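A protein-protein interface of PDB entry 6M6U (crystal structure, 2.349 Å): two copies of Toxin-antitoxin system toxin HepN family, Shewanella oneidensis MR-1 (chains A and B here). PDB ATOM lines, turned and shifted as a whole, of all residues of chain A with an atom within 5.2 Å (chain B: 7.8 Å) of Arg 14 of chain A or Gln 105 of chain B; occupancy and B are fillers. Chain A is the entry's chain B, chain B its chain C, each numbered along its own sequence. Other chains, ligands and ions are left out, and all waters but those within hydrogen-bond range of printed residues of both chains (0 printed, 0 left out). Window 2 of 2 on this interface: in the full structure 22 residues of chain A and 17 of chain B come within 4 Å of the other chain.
The backbone carbonyl oxygen (O) of Asn 7 of chain A lies within hydrogen-bond range of the side-chain hydroxyl (OG1) of Thr 11 of chain A, 3.2 Å away. The backbone carbonyl oxygen of Thr 11 of chain A lies within hydrogen-bond range of the side-chain sulfur of Cys 15 of chain A, at 3.1 Å. OG1 of Thr 11 of chain A is in hydrogen-bond range of NH2 of Arg 14 of chain A (3.1 Å). The backbone carbonyl oxygen (O) of Ile 99 of chain B sits at hydrogen-bond distance from the backbone NH (N) of Tyr 104 of chain B, 3.3 Å away.
Of the 11 printed residues of chain A, 3 touch a printed residue of chain B. Of the 11 printed residues of chain B, 2 touch a printed residue of chain A.
Of chain A, only Arg 14 comes within 4 Å of Gln 105 of chain B. Of the printed residues of chain A, Tyr 104 of chain B touches Thr 11, Arg 14 and Cys 15. Of the printed residues of chain B, Thr 11 of chain A touches Tyr 104. Printed residues of chain B within 4 Å of Cys 15 of chain A: Tyr 104 (3.5 Å). Ile 12 of chain A touches none of the printed residues of chain B. The nearest printed residue of chain B that does not touch Cys 15 of chain A is Gln 105 of chain B (7.1 Å).
No position is printed for both chains. Of the 4 pairs that touch across the chains among the printed residues, none has its exchanged pair printed and touching as well.
The guanidinium group of Arg 14 of chain A sits at hydrogen-bond distance from the side-chain hydroxyl of Tyr 104 of chain B, 2.7 Å away. The guanidinium group of Arg 14 of chain A lies close to the side-chain amide nitrogen of Gln 105 of chain B. OH of Tyr 104 of chain B is in hydrogen-bond range of SG of Cys 15 of chain A (3.5 Å).
Thr 11 of chain A touches Tyr 104 of chain B (CG2 to CE2, 3.6 Å).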
ATOM      1  N   ASN A   7     -15.510   7.327 -17.113  1.00  0.00           N
ATOM      2  CA  ASN A   7     -16.579   6.458 -16.625  1.00  0.00           C
ATOM      3  C   ASN A   7     -17.708   7.261 -15.992  1.00  0.00           C
ATOM      4  O   ASN A   7     -18.886   6.915 -16.150  1.00  0.00           O
ATOM      5  CB  ASN A   7     -16.022   5.435 -15.637  1.00  0.00           C
ATOM      6  CG  ASN A   7     -15.172   4.378 -16.315  1.00  0.00           C
ATOM      7  OD1 ASN A   7     -15.649   3.288 -16.630  1.00  0.00           O
ATOM      8  ND2 ASN A   7     -13.907   4.702 -16.555  1.00  0.00           N
ATOM      9  N   ILE A   9     -18.551  10.347 -16.830  1.00  0.00           N
ATOM     10  CA  ILE A   9     -19.261  10.892 -17.988  1.00  0.00           C
ATOM     11  C   ILE A   9     -20.254   9.870 -18.517  1.00  0.00           C
ATOM     12  O   ILE A   9     -21.441  10.164 -18.698  1.00  0.00           O
ATOM     13  CB  ILE A   9     -18.271  11.315 -19.088  1.00  0.00           C
ATOM     14  CG1 ILE A   9     -17.424  12.513 -18.653  1.00  0.00           C
ATOM     15  CG2 ILE A   9     -19.020  11.629 -20.379  1.00  0.00           C
ATOM     16  CD1 ILE A   9     -18.223  13.665 -18.114  1.00  0.00           C
ATOM     17  N   ALA A  10     -19.778   8.646 -18.764  1.00  0.00           N
ATOM     18  CA  ALA A  10     -20.645   7.595 -19.289  1.00  0.00           C
ATOM     19  C   ALA A  10     -21.848   7.358 -18.382  1.00  0.00           C
ATOM     20  O   ALA A  10     -22.963   7.125 -18.864  1.00  0.00           O
ATOM     21  CB  ALA A  10     -19.850   6.302 -19.470  1.00  0.00           C
ATOM     22  N   THR A  11     -21.644   7.429 -17.064  1.00  0.00           N
ATOM     23  CA  THR A  11     -22.742   7.193 -16.130  1.00  0.00           C
ATOM     24  C   THR A  11     -23.783   8.304 -16.200  1.00  0.00           C
ATOM     25  O   THR A  11     -24.989   8.029 -16.185  1.00  0.00           O
ATOM     26  CB  THR A  11     -22.194   7.044 -14.711  1.00  0.00           C
ATOM     27  OG1 THR A  11     -21.512   5.790 -14.607  1.00  0.00           O
ATOM     28  CG2 THR A  11     -23.316   7.098 -13.680  1.00  0.00           C
ATOM     29  N   ILE A  12     -23.341   9.563 -16.278  1.00  0.00           N
ATOM     30  CA  ILE A  12     -24.278  10.676 -16.413  1.00  0.00           C
ATOM     31  C   ILE A  12     -25.135  10.498 -17.661  1.00  0.00           C
ATOM     32  O   ILE A  12     -26.358  10.682 -17.629  1.00  0.00           O
ATOM     33  CB  ILE A  12     -23.526  12.018 -16.435  1.00  0.00           C
ATOM     34  CG1 ILE A  12     -22.844  12.265 -15.091  1.00  0.00           C
ATOM     35  CG2 ILE A  12     -24.482  13.160 -16.772  1.00  0.00           C
ATOM     36  CD1 ILE A  12     -21.823  13.378 -15.110  1.00  0.00           C
ATOM     37  N   LYS A  13     -24.505  10.119 -18.775  1.00  0.00           N
ATOM     38  CA  LYS A  13     -25.249   9.904 -20.013  1.00  0.00           C
ATOM     39  C   LYS A  13     -26.250   8.765 -19.866  1.00  0.00           C
ATOM     40  O   LYS A  13     -27.435   8.924 -20.183  1.00  0.00           O
ATOM     41  CB  LYS A  13     -24.287   9.634 -21.168  1.00  0.00           C
ATOM     42  CG  LYS A  13     -23.581  10.876 -21.669  1.00  0.00           C
ATOM     43  CD  LYS A  13     -22.464  10.535 -22.634  1.00  0.00           C
ATOM     44  CE  LYS A  13     -21.832  11.798 -23.190  1.00  0.00           C
ATOM     45  NZ  LYS A  13     -20.555  11.514 -23.902  1.00  0.00           N
ATOM     46  N   ARG A  14     -25.790   7.603 -19.385  1.00  0.00           N
ATOM     47  CA  ARG A  14     -26.693   6.472 -19.184  1.00  0.00           C
ATOM     48  C   ARG A  14     -27.882   6.855 -18.317  1.00  0.00           C
ATOM     49  O   ARG A  14     -29.012   6.433 -18.579  1.00  0.00           O
ATOM     50  CB  ARG A  14     -25.954   5.296 -18.544  1.00  0.00           C
ATOM     51  CG  ARG A  14     -25.258   4.367 -19.516  1.00  0.00           C
ATOM     52  CD  ARG A  14     -25.046   2.993 -18.890  1.00  0.00           C
ATOM     53  NE  ARG A  14     -24.699   3.077 -17.473  1.00  0.00           N
ATOM     54  CZ  ARG A  14     -23.508   3.453 -17.010  1.00  0.00           C
ATOM     55  NH1 ARG A  14     -22.539   3.788 -17.853  1.00  0.00           N
ATOM     56  NH2 ARG A  14     -23.287   3.499 -15.702  1.00  0.00           N
ATOM     57  N   CYS A  15     -27.650   7.669 -17.287  1.00  0.00           N
ATOM     58  CA  CYS A  15     -28.720   7.973 -16.347  1.00  0.00           C
ATOM     59  C   CYS A  15     -29.660   9.062 -16.854  1.00  0.00           C
ATOM     60  O   CYS A  15     -30.841   9.061 -16.491  1.00  0.00           O
ATOM     61  CB  CYS A  15     -28.131   8.365 -14.995  1.00  0.00           C
ATOM     62  SG  CYS A  15     -27.213   7.022 -14.238  1.00  0.00           S
ATOM     63  N   ILE A  16     -29.173   9.997 -17.679  1.00  0.00           N
ATOM     64  CA  ILE A  16     -30.069  10.986 -18.283  1.00  0.00           C
ATOM     65  C   ILE A  16     -31.021  10.307 -19.258  1.00  0.00           C
ATOM     66  O   ILE A  16     -32.223  10.608 -19.295  1.00  0.00           O
ATOM     67  CB  ILE A  16     -29.272  12.106 -18.976  1.00  0.00           C
ATOM     68  CG1 ILE A  16     -28.559  12.982 -17.947  1.00  0.00           C
ATOM     69  CG2 ILE A  16     -30.195  12.972 -19.828  1.00  0.00           C
ATOM     70  CD1 ILE A  16     -27.839  14.155 -18.566  1.00  0.00           C
ATOM     71  N   LYS A  17     -30.498   9.374 -20.064  1.00  0.00           N
ATOM     72  CA  LYS A  17     -31.371   8.596 -20.941  1.00  0.00           C
ATOM     73  C   LYS A  17     -32.364   7.769 -20.134  1.00  0.00           C
ATOM     74  O   LYS A  17     -33.534   7.653 -20.514  1.00  0.00           O
ATOM     75  CB  LYS A  17     -30.551   7.697 -21.866  1.00  0.00           C
ATOM     76  CG  LYS A  17     -29.655   8.451 -22.837  1.00  0.00           C
ATOM     77  CD  LYS A  17     -29.517   7.705 -24.165  1.00  0.00           C
ATOM     78  CE  LYS A  17     -28.693   6.434 -24.023  1.00  0.00           C
ATOM     79  NZ  LYS A  17     -27.259   6.715 -23.709  1.00  0.00           N
ATOM     80  N   ARG A  18     -31.919   7.192 -19.011  1.00  0.00           N
ATOM     81  CA  ARG A  18     -32.844   6.490 -18.127  1.00  0.00           C
ATOM     82  C   ARG A  18     -33.950   7.415 -17.632  1.00  0.00           C
ATOM     83  O   ARG A  18     -35.098   6.982 -17.473  1.00  0.00           O
ATOM     84  CB  ARG A  18     -32.088   5.879 -16.943  1.00  0.00           C
ATOM     85  CG  ARG A  18     -31.371   4.578 -17.264  1.00  0.00           C
ATOM     86  CD  ARG A  18     -32.370   3.492 -17.618  1.00  0.00           C
ATOM     87  NE  ARG A  18     -33.274   3.204 -16.507  1.00  0.00           N
ATOM     88  CZ  ARG A  18     -34.510   2.734 -16.649  1.00  0.00           C
ATOM     89  NH1 ARG A  18     -35.001   2.504 -17.859  1.00  0.00           N
ATOM     90  NH2 ARG A  18     -35.259   2.500 -15.579  1.00  0.00           N
ATOM     91  N   ILE B  99     -22.874   1.200  -1.749  1.00  0.00           N
ATOM     92  CA  ILE B  99     -22.689   0.777  -3.130  1.00  0.00           C
ATOM     93  C   ILE B  99     -23.761   1.396  -4.027  1.00  0.00           C
ATOM     94  O   ILE B  99     -23.466   1.859  -5.133  1.00  0.00           O
ATOM     95  CB  ILE B  99     -22.678  -0.760  -3.213  1.00  0.00           C
ATOM     96  CG1 ILE B  99     -21.550  -1.315  -2.339  1.00  0.00           C
ATOM     97  CG2 ILE B  99     -22.514  -1.222  -4.649  1.00  0.00           C
ATOM     98  CD1 ILE B  99     -21.410  -2.821  -2.388  1.00  0.00           C
ATOM     99  N   ALA B 100     -25.011   1.443  -3.556  1.00  0.00           N
ATOM    100  CA  ALA B 100     -26.096   1.961  -4.386  1.00  0.00           C
ATOM    101  C   ALA B 100     -25.912   3.445  -4.698  1.00  0.00           C
ATOM    102  O   ALA B 100     -26.252   3.901  -5.796  1.00  0.00           O
ATOM    103  CB  ALA B 100     -27.442   1.726  -3.701  1.00  0.00           C
ATOM    104  N   VAL B 101     -25.372   4.214  -3.751  1.00  0.00           N
ATOM    105  CA  VAL B 101     -25.273   5.659  -3.933  1.00  0.00           C
ATOM    106  C   VAL B 101     -24.015   6.031  -4.710  1.00  0.00           C
ATOM    107  O   VAL B 101     -24.053   6.875  -5.615  1.00  0.00           O
ATOM    108  CB  VAL B 101     -25.323   6.374  -2.568  1.00  0.00           C
ATOM    109  CG1 VAL B 101     -25.079   7.868  -2.736  1.00  0.00           C
ATOM    110  CG2 VAL B 101     -26.660   6.125  -1.887  1.00  0.00           C
ATOM    111  N   HIS B 102     -22.881   5.415  -4.374  1.00  0.00           N
ATOM    112  CA  HIS B 102     -21.608   5.848  -4.938  1.00  0.00           C
ATOM    113  C   HIS B 102     -21.270   5.146  -6.249  1.00  0.00           C
ATOM    114  O   HIS B 102     -20.710   5.776  -7.152  1.00  0.00           O
ATOM    115  CB  HIS B 102     -20.480   5.631  -3.924  1.00  0.00           C
ATOM    116  CG  HIS B 102     -20.736   6.258  -2.584  1.00  0.00           C
ATOM    117  ND1 HIS B 102     -21.017   7.598  -2.427  1.00  0.00           N
ATOM    118  CD2 HIS B 102     -20.751   5.724  -1.339  1.00  0.00           C
ATOM    119  CE1 HIS B 102     -21.201   7.861  -1.146  1.00  0.00           C
ATOM    120  NE2 HIS B 102     -21.045   6.742  -0.464  1.00  0.00           N
ATOM    121  N   ASP B 103     -21.595   3.852  -6.379  1.00  0.00           N
ATOM    122  CA  ASP B 103     -21.255   3.101  -7.594  1.00  0.00           C
ATOM    123  C   ASP B 103     -22.367   2.073  -7.838  1.00  0.00           C
ATOM    124  O   ASP B 103     -22.229   0.877  -7.565  1.00  0.00           O
ATOM    125  CB  ASP B 103     -19.885   2.435  -7.487  1.00  0.00           C
ATOM    126  CG  ASP B 103     -19.422   1.843  -8.803  1.00  0.00           C
ATOM    127  OD1 ASP B 103     -18.597   0.907  -8.773  1.00  0.00           O
ATOM    128  OD2 ASP B 103     -19.883   2.313  -9.867  1.00  0.00           O
ATOM    129  N   TYR B 104     -23.482   2.560  -8.388  1.00  0.00           N
ATOM    130  CA  TYR B 104     -24.696   1.755  -8.466  1.00  0.00           C
ATOM    131  C   TYR B 104     -24.542   0.561  -9.395  1.00  0.00           C
ATOM    132  O   TYR B 104     -25.217  -0.457  -9.206  1.00  0.00           O
ATOM    133  CB  TYR B 104     -25.856   2.621  -8.939  1.00  0.00           C
ATOM    134  CG  TYR B 104     -25.809   2.949 -10.421  1.00  0.00           C
ATOM    135  CD1 TYR B 104     -26.490   2.164 -11.351  1.00  0.00           C
ATOM    136  CD2 TYR B 104     -25.094   4.045 -10.889  1.00  0.00           C
ATOM    137  CE1 TYR B 104     -26.458   2.463 -12.697  1.00  0.00           C
ATOM    138  CE2 TYR B 104     -25.057   4.349 -12.237  1.00  0.00           C
ATOM    139  CZ  TYR B 104     -25.740   3.553 -13.136  1.00  0.00           C
ATOM    140  OH  TYR B 104     -25.708   3.845 -14.481  1.00  0.00           O
ATOM    141  N   GLN B 105     -23.692   0.674 -10.418  1.00  0.00           N
ATOM    142  CA  GLN B 105     -23.551  -0.400 -11.395  1.00  0.00           C
ATOM    143  C   GLN B 105     -23.057  -1.694 -10.768  1.00  0.00           C
ATOM    144  O   GLN B 105     -23.317  -2.773 -11.314  1.00  0.00           O
ATOM    145  CB  GLN B 105     -22.604   0.031 -12.516  1.00  0.00           C
ATOM    146  CG  GLN B 105     -23.279   0.792 -13.644  1.00  0.00           C
ATOM    147  CD  GLN B 105     -23.970  -0.127 -14.635  1.00  0.00           C
ATOM    148  OE1 GLN B 105     -23.716  -1.333 -14.664  1.00  0.00           O
ATOM    149  NE2 GLN B 105     -24.851   0.438 -15.454  1.00  0.00           N
ATOM    150  N   GLU B 106     -22.370  -1.616  -9.632  1.00  0.00           N
ATOM    151  CA  GLU B 106     -21.819  -2.790  -8.973  1.00  0.00           C
ATOM    152  C   GLU B 106     -22.768  -3.402  -7.949  1.00  0.00           C
ATOM    153  O   GLU B 106     -22.357  -4.293  -7.199  1.00  0.00           O
ATOM    154  CB  GLU B 106     -20.487  -2.440  -8.308  1.00  0.00           C
ATOM    155  CG  GLU B 106     -19.393  -2.088  -9.303  1.00  0.00           C
ATOM    156  CD  GLU B 106     -19.153  -3.192 -10.316  1.00  0.00           C
ATOM    157  OE1 GLU B 106     -19.010  -4.361  -9.898  1.00  0.00           O
ATOM    158  OE2 GLU B 106     -19.117  -2.894 -11.529  1.00  0.00           O
ATOM    159  N   LEU B 107     -24.016  -2.946  -7.895  1.00  0.00           N
ATOM    160  CA  LEU B 107     -25.005  -3.602  -7.055  1.00  0.00           C
ATOM    161  C   LEU B 107     -25.262  -5.014  -7.562  1.00  0.00           C
ATOM    162  O   LEU B 107     -25.369  -5.250  -8.770  1.00  0.00           O
ATOM    163  CB  LEU B 107     -26.312  -2.808  -7.039  1.00  0.00           C
ATOM    164  CG  LEU B 107     -26.382  -1.549  -6.174  1.00  0.00           C
ATOM    165  CD1 LEU B 107     -27.699  -0.827  -6.405  1.00  0.00           C
ATOM    166  CD2 LEU B 107     -26.217  -1.907  -4.707  1.00  0.00           C
ATOM    167  N   ASN B 108     -25.345  -5.962  -6.634  1.00  0.00           N
ATOM    168  CA  ASN B 108     -25.709  -7.333  -6.967  1.00  0.00           C
ATOM    169  C   ASN B 108     -27.209  -7.490  -6.746  1.00  0.00           C
ATOM    170  O   ASN B 108     -27.676  -7.516  -5.604  1.00  0.00           O
ATOM    171  CB  ASN B 108     -24.902  -8.320  -6.132  1.00  0.00           C
ATOM    172  CG  ASN B 108     -25.182  -9.768  -6.492  1.00  0.00           C
ATOM    173  OD1 ASN B 108     -26.009 -10.066  -7.354  1.00  0.00           O
ATOM    174  ND2 ASN B 108     -24.461 -10.678  -5.854  1.00  0.00           N
ATOM    175  N   LEU B 109     -27.956  -7.602  -7.850  1.00  0.00           N
ATOM    176  CA  LEU B 109     -29.408  -7.733  -7.777  1.00  0.00           C
ATOM    177  C   LEU B 109     -29.828  -8.911  -6.916  1.00  0.00           C
ATOM    178  O   LEU B 109     -30.878  -8.864  -6.265  1.00  0.00           O
ATOM    179  CB  LEU B 109     -29.987  -7.888  -9.184  1.00  0.00           C
ATOM    180  CG  LEU B 109     -30.041  -6.633 -10.051  1.00  0.00           C
ATOM    181  CD1 LEU B 109     -30.411  -6.985 -11.488  1.00  0.00           C
ATOM    182  CD2 LEU B 109     -31.031  -5.639  -9.465  1.00  0.00           C
